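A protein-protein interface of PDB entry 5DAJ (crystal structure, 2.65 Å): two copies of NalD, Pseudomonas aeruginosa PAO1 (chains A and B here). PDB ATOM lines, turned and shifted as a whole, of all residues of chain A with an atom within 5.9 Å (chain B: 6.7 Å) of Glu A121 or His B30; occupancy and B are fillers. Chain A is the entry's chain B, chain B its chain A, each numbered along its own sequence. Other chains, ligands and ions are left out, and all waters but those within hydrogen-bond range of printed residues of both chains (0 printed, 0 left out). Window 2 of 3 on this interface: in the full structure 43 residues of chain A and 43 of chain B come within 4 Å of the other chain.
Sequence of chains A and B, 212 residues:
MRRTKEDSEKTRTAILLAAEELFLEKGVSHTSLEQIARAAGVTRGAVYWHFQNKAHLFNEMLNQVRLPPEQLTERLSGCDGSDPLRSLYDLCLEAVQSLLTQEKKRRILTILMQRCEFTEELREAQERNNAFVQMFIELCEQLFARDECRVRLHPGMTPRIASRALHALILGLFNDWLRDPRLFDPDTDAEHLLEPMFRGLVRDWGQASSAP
O of Lys B26 sits close to OG1 of Thr A119. The side-chain carboxylate (OE1) of Glu A117 sits at hydrogen-bond distance from the backbone NH (N) of Val B28. N of Ser B29 is in hydrogen-bond range of OE1 of Glu A117 (2.8 Å). The backbone NH (N) of His B30 is in hydrogen-bond range of the side-chain carboxylate (OE2) of Glu A117 (3.4 Å).
The side-chain amide nitrogen (NE2) of Gln B35 lies close to the side-chain amino group (NZ) of Lys B26 (3.4 Å). The backbone carbonyl oxygen (O) of Gly B27 lies within hydrogen-bond range of the side-chain hydroxyl (OG1) of Thr B31 (2.6 Å). The backbone carbonyl oxygen of His B30 lies close to the side-chain amide oxygen of Gln B35. The side-chain carboxylate of Glu B121 lies within salt-bridge range of the side-chain amino group of Lys B54 (3.2 Å). OG of Ser A29 lies close to OE2 of Glu A117 (3.3 Å). The side-chain amino group (NZ) of Lys A54 lies within salt-bridge range of the side-chain carboxylate (OE2) of Glu A121, at 3.2 Å.
Among the printed residues, merely in contact across the chains: Ser A29 with Ser B29 (3.3 Å), Glu A117 with Gly B27 (3.5 Å), Glu A121 with His B30 (3.5 Å), Ser A29 with His B30 (3.5 Å), His A30 with Glu B121 (3.6 Å) and His A30 with Ser B29 (3.9 Å).
Of the printed residues of chain B, Glu A117 touches Gly B27 (3.5 Å), Val B28 (3.2 Å), Ser B29 (2.8 Å) and His B30 (3.4 Å). Printed residues of chain B within 4 Å of Thr A119: Lys B26 (3.0 Å). Glu A121 touches just one residue of chain B: His B30. Of chain A, only Ser A29 (3.5 Å), Glu A117 (3.4 Å) and Glu A121 (3.5 Å) come within 4 Å of His B30. Thr B31 touches none of the printed residues of chain A. The nearest printed residue of chain B that does not touch Glu A121 is Lys B26 (7.5 Å).
Hydrophobic or aromatic side chains of chain A within 4 Å of the printed part of chain B: His A30. Printed residues of chain B that touch a printed residue of chain A: Lys B26, Gly B27, Val B28, Ser B29, His B30 and Glu B121. Hydrophobic or aromatic side chains of chain B within 4 Å of the printed part of chain A: Val B28 and His B30. Among the printed residues, no Asp or Glu carboxylate lies within 4 Å of a Lys or Arg side-chain nitrogen of the other chain.
Ser B29 touches its own counterpart, Ser A29. Ser A29 touches His B30, and with the chains exchanged His A30 touches Ser B29. His A30 touches Glu B121, and with the chains exchanged Glu A121 touches His B30. 5 positions are printed for both chains. Of the 10 pairs that touch across the chains among the printed residues, 5 have their exchanged pair printed and touching as well.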
ATOM      1  N   VAL A  28      23.550  -0.586  13.982  1.00  0.00           N
ATOM      2  CA  VAL A  28      23.511  -1.969  13.468  1.00  0.00           C
ATOM      3  C   VAL A  28      22.348  -2.788  14.045  1.00  0.00           C
ATOM      4  O   VAL A  28      21.682  -3.521  13.307  1.00  0.00           O
ATOM      5  CB  VAL A  28      24.853  -2.699  13.717  1.00  0.00           C
ATOM      6  CG1 VAL A  28      24.761  -4.186  13.381  1.00  0.00           C
ATOM      7  CG2 VAL A  28      25.951  -2.060  12.875  1.00  0.00           C
ATOM      8  N   SER A  29      22.134  -2.673  15.356  1.00  0.00           N
ATOM      9  CA  SER A  29      21.049  -3.380  16.067  1.00  0.00           C
ATOM     10  C   SER A  29      19.677  -3.109  15.457  1.00  0.00           C
ATOM     11  O   SER A  29      18.923  -4.031  15.145  1.00  0.00           O
ATOM     12  CB  SER A  29      21.017  -2.961  17.531  1.00  0.00           C
ATOM     13  OG  SER A  29      22.129  -3.486  18.228  1.00  0.00           O
ATOM     14  N   HIS A  30      19.389  -1.825  15.270  1.00  0.00           N
ATOM     15  CA  HIS A  30      18.123  -1.344  14.694  1.00  0.00           C
ATOM     16  C   HIS A  30      18.057  -1.405  13.152  1.00  0.00           C
ATOM     17  O   HIS A  30      17.105  -0.899  12.555  1.00  0.00           O
ATOM     18  CB  HIS A  30      17.844   0.088  15.186  1.00  0.00           C
ATOM     19  CG  HIS A  30      17.598   0.183  16.663  1.00  0.00           C
ATOM     20  ND1 HIS A  30      16.572  -0.487  17.295  1.00  0.00           N
ATOM     21  CD2 HIS A  30      18.246   0.873  17.631  1.00  0.00           C
ATOM     22  CE1 HIS A  30      16.598  -0.215  18.587  1.00  0.00           C
ATOM     23  NE2 HIS A  30      17.604   0.610  18.818  1.00  0.00           N
ATOM     24  N   ASN A  53      24.149 -14.035   7.021  1.00  0.00           N
ATOM     25  CA  ASN A  53      23.649 -13.374   8.232  1.00  0.00           C
ATOM     26  C   ASN A  53      24.241 -11.984   8.407  1.00  0.00           C
ATOM     27  O   ASN A  53      25.186 -11.615   7.706  1.00  0.00           O
ATOM     28  CB  ASN A  53      23.945 -14.243   9.455  1.00  0.00           C
ATOM     29  CG  ASN A  53      25.431 -14.477   9.660  1.00  0.00           C
ATOM     30  OD1 ASN A  53      26.168 -13.559  10.017  1.00  0.00           O
ATOM     31  ND2 ASN A  53      25.879 -15.708   9.446  1.00  0.00           N
ATOM     32  N   LYS A  54      23.699 -11.241   9.367  1.00  0.00           N
ATOM     33  CA  LYS A  54      24.097  -9.850   9.603  1.00  0.00           C
ATOM     34  C   LYS A  54      25.569  -9.707   9.992  1.00  0.00           C
ATOM     35  O   LYS A  54      26.245  -8.783   9.541  1.00  0.00           O
ATOM     36  CB  LYS A  54      23.224  -9.197  10.683  1.00  0.00           C
ATOM     37  CG  LYS A  54      23.289  -7.674  10.654  1.00  0.00           C
ATOM     38  CD  LYS A  54      22.759  -7.020  11.915  1.00  0.00           C
ATOM     39  CE  LYS A  54      21.267  -7.192  12.061  1.00  0.00           C
ATOM     40  NZ  LYS A  54      20.751  -6.320  13.149  1.00  0.00           N
ATOM     41  N   ALA A  55      26.054 -10.615  10.834  1.00  0.00           N
ATOM     42  CA  ALA A  55      27.451 -10.589  11.306  1.00  0.00           C
ATOM     43  C   ALA A  55      28.443 -10.774  10.173  1.00  0.00           C
ATOM     44  O   ALA A  55      29.471 -10.095  10.123  1.00  0.00           O
ATOM     45  CB  ALA A  55      27.682 -11.656  12.368  1.00  0.00           C
ATOM     46  N   GLU A 117      26.899  -2.573  18.617  1.00  0.00           N
ATOM     47  CA  GLU A 117      27.100  -3.200  19.923  1.00  0.00           C
ATOM     48  C   GLU A 117      27.313  -4.684  19.701  1.00  0.00           C
ATOM     49  O   GLU A 117      26.564  -5.329  18.960  1.00  0.00           O
ATOM     50  CB  GLU A 117      25.926  -2.937  20.886  1.00  0.00           C
ATOM     51  CG  GLU A 117      24.532  -3.103  20.308  1.00  0.00           C
ATOM     52  CD  GLU A 117      23.443  -2.701  21.290  1.00  0.00           C
ATOM     53  OE1 GLU A 117      23.478  -1.555  21.799  1.00  0.00           O
ATOM     54  OE2 GLU A 117      22.506  -3.511  21.522  1.00  0.00           O
ATOM     55  N   THR A 119      26.749  -7.800  20.712  1.00  0.00           N
ATOM     56  CA  THR A 119      25.893  -8.858  21.270  1.00  0.00           C
ATOM     57  C   THR A 119      26.284 -10.226  20.679  1.00  0.00           C
ATOM     58  O   THR A 119      27.255 -10.340  19.928  1.00  0.00           O
ATOM     59  CB  THR A 119      24.390  -8.538  20.995  1.00  0.00           C
ATOM     60  OG1 THR A 119      24.201  -7.123  21.037  1.00  0.00           O
ATOM     61  CG2 THR A 119      23.414  -9.184  22.007  1.00  0.00           C
ATOM     62  N   GLU A 120      25.556 -11.269  21.072  1.00  0.00           N
ATOM     63  CA  GLU A 120      25.662 -12.602  20.457  1.00  0.00           C
ATOM     64  C   GLU A 120      25.481 -12.585  18.938  1.00  0.00           C
ATOM     65  O   GLU A 120      26.231 -13.246  18.227  1.00  0.00           O
ATOM     66  CB  GLU A 120      24.637 -13.567  21.063  1.00  0.00           C
ATOM     67  CG  GLU A 120      24.878 -15.032  20.719  1.00  0.00           C
ATOM     68  CD  GLU A 120      25.802 -15.724  21.704  1.00  0.00           C
ATOM     69  OE1 GLU A 120      25.390 -15.918  22.869  1.00  0.00           O
ATOM     70  OE2 GLU A 120      26.931 -16.086  21.313  1.00  0.00           O
ATOM     71  N   GLU A 121      24.509 -11.823  18.435  1.00  0.00           N
ATOM     72  CA  GLU A 121      24.219 -11.835  16.986  1.00  0.00           C
ATOM     73  C   GLU A 121      25.389 -11.322  16.122  1.00  0.00           C
ATOM     74  O   GLU A 121      25.437 -11.605  14.926  1.00  0.00           O
ATOM     75  CB  GLU A 121      22.889 -11.121  16.644  1.00  0.00           C
ATOM     76  CG  GLU A 121      22.929  -9.603  16.455  1.00  0.00           C
ATOM     77  CD  GLU A 121      21.651  -9.028  15.845  1.00  0.00           C
ATOM     78  OE1 GLU A 121      20.798  -9.800  15.339  1.00  0.00           O
ATOM     79  OE2 GLU A 121      21.496  -7.784  15.859  1.00  0.00           O
ATOM     80  N   LEU A 122      26.306 -10.569  16.730  1.00  0.00           N
ATOM     81  CA  LEU A 122      27.558 -10.143  16.072  1.00  0.00           C
ATOM     82  C   LEU A 122      28.814 -10.849  16.615  1.00  0.00           C
ATOM     83  O   LEU A 122      29.917 -10.310  16.529  1.00  0.00           O
ATOM     84  CB  LEU A 122      27.715  -8.617  16.160  1.00  0.00           C
ATOM     85  CG  LEU A 122      26.773  -7.829  15.246  1.00  0.00           C
ATOM     86  CD1 LEU A 122      25.703  -7.105  16.049  1.00  0.00           C
ATOM     87  CD2 LEU A 122      27.562  -6.832  14.418  1.00  0.00           C
ATOM     88  N   ARG A 123      28.644 -12.054  17.152  1.00  0.00           N
ATOM     89  CA  ARG A 123      29.759 -12.845  17.703  1.00  0.00           C
ATOM     90  C   ARG A 123      30.861 -13.055  16.669  1.00  0.00           C
ATOM     91  O   ARG A 123      32.033 -12.805  16.950  1.00  0.00           O
ATOM     92  CB  ARG A 123      29.270 -14.214  18.188  1.00  0.00           C
ATOM     93  CG  ARG A 123      30.253 -14.954  19.085  1.00  0.00           C
ATOM     94  CD  ARG A 123      30.030 -14.637  20.557  1.00  0.00           C
ATOM     95  NE  ARG A 123      31.017 -15.322  21.426  1.00  0.00           N
ATOM     96  CZ  ARG A 123      32.339 -15.072  21.505  1.00  0.00           C
ATOM     97  NH1 ARG A 123      32.932 -14.137  20.756  1.00  0.00           N
ATOM     98  NH2 ARG A 123      33.100 -15.782  22.353  1.00  0.00           N
ATOM     99  N   GLU A 124      30.457 -13.497  15.479  1.00  0.00           N
ATOM    100  CA  GLU A 124      31.375 -13.771  14.360  1.00  0.00           C
ATOM    101  C   GLU A 124      32.224 -12.560  13.980  1.00  0.00           C
ATOM    102  O   GLU A 124      33.428 -12.687  13.716  1.00  0.00           O
ATOM    103  CB  GLU A 124      30.592 -14.231  13.129  1.00  0.00           C
ATOM    104  CG  GLU A 124      31.453 -14.554  11.911  1.00  0.00           C
ATOM    105  CD  GLU A 124      30.643 -14.834  10.652  1.00  0.00           C
ATOM    106  OE1 GLU A 124      29.454 -15.227  10.748  1.00  0.00           O
ATOM    107  OE2 GLU A 124      31.210 -14.660   9.553  1.00  0.00           O
ATOM    108  N   LEU B  22      21.749  -6.131  32.394  1.00  0.00           N
ATOM    109  CA  LEU B  22      21.070  -6.321  31.095  1.00  0.00           C
ATOM    110  C   LEU B  22      21.860  -5.751  29.917  1.00  0.00           C
ATOM    111  O   LEU B  22      22.064  -6.447  28.918  1.00  0.00           O
ATOM    112  CB  LEU B  22      19.655  -5.738  31.088  1.00  0.00           C
ATOM    113  CG  LEU B  22      18.559  -6.737  31.463  1.00  0.00           C
ATOM    114  CD1 LEU B  22      18.392  -6.815  32.969  1.00  0.00           C
ATOM    115  CD2 LEU B  22      17.245  -6.353  30.812  1.00  0.00           C
ATOM    116  N   LYS B  26      22.922  -8.166  27.000  1.00  0.00           N
ATOM    117  CA  LYS B  26      22.110  -8.030  25.774  1.00  0.00           C
ATOM    118  C   LYS B  26      22.562  -6.920  24.829  1.00  0.00           C
ATOM    119  O   LYS B  26      22.248  -6.950  23.636  1.00  0.00           O
ATOM    120  CB  LYS B  26      20.644  -7.773  26.148  1.00  0.00           C
ATOM    121  CG  LYS B  26      19.922  -8.977  26.736  1.00  0.00           C
ATOM    122  CD  LYS B  26      18.758  -8.572  27.643  1.00  0.00           C
ATOM    123  CE  LYS B  26      17.741  -7.653  26.968  1.00  0.00           C
ATOM    124  NZ  LYS B  26      17.005  -8.314  25.855  1.00  0.00           N
ATOM    125  N   GLY B  27      23.260  -5.930  25.371  1.00  0.00           N
ATOM    126  CA  GLY B  27      23.530  -4.686  24.652  1.00  0.00           C
ATOM    127  C   GLY B  27      22.468  -3.655  24.973  1.00  0.00           C
ATOM    128  O   GLY B  27      21.367  -4.004  25.388  1.00  0.00           O
ATOM    129  N   VAL B  28      22.788  -2.385  24.760  1.00  0.00           N
ATOM    130  CA  VAL B  28      21.889  -1.274  25.108  1.00  0.00           C
ATOM    131  C   VAL B  28      20.678  -1.175  24.170  1.00  0.00           C
ATOM    132  O   VAL B  28      19.560  -0.961  24.631  1.00  0.00           O
ATOM    133  CB  VAL B  28      22.644   0.079  25.152  1.00  0.00           C
ATOM    134  CG1 VAL B  28      21.691   1.263  25.307  1.00  0.00           C
ATOM    135  CG2 VAL B  28      23.637   0.081  26.303  1.00  0.00           C
ATOM    136  N   SER B  29      20.916  -1.303  22.867  1.00  0.00           N
ATOM    137  CA  SER B  29      19.856  -1.241  21.843  1.00  0.00           C
ATOM    138  C   SER B  29      18.739  -2.249  22.101  1.00  0.00           C
ATOM    139  O   SER B  29      17.558  -1.901  22.104  1.00  0.00           O
ATOM    140  CB  SER B  29      20.439  -1.511  20.454  1.00  0.00           C
ATOM    141  OG  SER B  29      21.228  -0.423  20.031  1.00  0.00           O
ATOM    142  N   HIS B  30      19.149  -3.496  22.316  1.00  0.00           N
ATOM    143  CA  HIS B  30      18.239  -4.623  22.574  1.00  0.00           C
ATOM    144  C   HIS B  30      17.736  -4.706  24.027  1.00  0.00           C
ATOM    145  O   HIS B  30      17.102  -5.692  24.401  1.00  0.00           O
ATOM    146  CB  HIS B  30      18.919  -5.947  22.165  1.00  0.00           C
ATOM    147  CG  HIS B  30      19.175  -6.062  20.692  1.00  0.00           C
ATOM    148  ND1 HIS B  30      18.164  -6.015  19.753  1.00  0.00           N
ATOM    149  CD2 HIS B  30      20.325  -6.230  19.997  1.00  0.00           C
ATOM    150  CE1 HIS B  30      18.683  -6.146  18.545  1.00  0.00           C
ATOM    151  NE2 HIS B  30      19.992  -6.278  18.666  1.00  0.00           N
ATOM    152  N   THR B  31      18.024  -3.686  24.837  1.00  0.00           N
ATOM    153  CA  THR B  31      17.509  -3.582  26.203  1.00  0.00           C
ATOM    154  C   THR B  31      16.546  -2.401  26.302  1.00  0.00           C
ATOM    155  O   THR B  31      16.927  -1.246  26.086  1.00  0.00           O
ATOM    156  CB  THR B  31      18.630  -3.387  27.241  1.00  0.00           C
ATOM    157  OG1 THR B  31      19.554  -4.472  27.142  1.00  0.00           O
ATOM    158  CG2 THR B  31      18.060  -3.352  28.668  1.00  0.00           C
ATOM    159  N   SER B  32      15.305  -2.708  26.660  1.00  0.00           N
ATOM    160  CA  SER B  32      14.259  -1.705  26.811  1.00  0.00           C
ATOM    161  C   SER B  32      14.087  -1.306  28.270  1.00  0.00           C
ATOM    162  O   SER B  32      14.571  -1.982  29.186  1.00  0.00           O
ATOM    163  CB  SER B  32      12.934  -2.257  26.287  1.00  0.00           C
ATOM    164  OG  SER B  32      12.451  -3.274  27.145  1.00  0.00           O
ATOM    165  N   GLN B  35      11.938  -3.989  30.032  1.00  0.00           N
ATOM    166  CA  GLN B  35      12.779  -5.124  30.445  1.00  0.00           C
ATOM    167  C   GLN B  35      13.604  -4.833  31.701  1.00  0.00           C
ATOM    168  O   GLN B  35      13.793  -5.708  32.552  1.00  0.00           O
ATOM    169  CB  GLN B  35      13.717  -5.526  29.317  1.00  0.00           C
ATOM    170  CG  GLN B  35      13.013  -6.216  28.163  1.00  0.00           C
ATOM    171  CD  GLN B  35      13.881  -6.340  26.921  1.00  0.00           C
ATOM    172  OE1 GLN B  35      14.646  -5.435  26.592  1.00  0.00           O
ATOM    173  NE2 GLN B  35      13.735  -7.444  26.204  1.00  0.00           N
ATOM    174  N   LYS B  54      16.035   6.373  28.231  1.00  0.00           N
ATOM    175  CA  LYS B  54      17.163   5.436  28.242  1.00  0.00           C
ATOM    176  C   LYS B  54      18.521   6.140  28.284  1.00  0.00           C
ATOM    177  O   LYS B  54      19.437   5.684  28.961  1.00  0.00           O
ATOM    178  CB  LYS B  54      17.107   4.486  27.029  1.00  0.00           C
ATOM    179  CG  LYS B  54      17.954   3.230  27.212  1.00  0.00           C
ATOM    180  CD  LYS B  54      18.202   2.471  25.928  1.00  0.00           C
ATOM    181  CE  LYS B  54      16.952   1.828  25.392  1.00  0.00           C
ATOM    182  NZ  LYS B  54      17.285   0.891  24.285  1.00  0.00           N
ATOM    183  N   GLU B 121      18.785   7.924  19.723  1.00  0.00           N
ATOM    184  CA  GLU B 121      18.165   7.675  21.037  1.00  0.00           C
ATOM    185  C   GLU B 121      19.153   7.806  22.212  1.00  0.00           C
ATOM    186  O   GLU B 121      18.726   7.995  23.342  1.00  0.00           O
ATOM    187  CB  GLU B 121      17.381   6.342  21.083  1.00  0.00           C
ATOM    188  CG  GLU B 121      18.170   5.073  21.399  1.00  0.00           C
ATOM    189  CD  GLU B 121      17.285   3.854  21.700  1.00  0.00           C
ATOM    190  OE1 GLU B 121      16.057   4.014  21.901  1.00  0.00           O
ATOM    191  OE2 GLU B 121      17.832   2.720  21.745  1.00  0.00           O
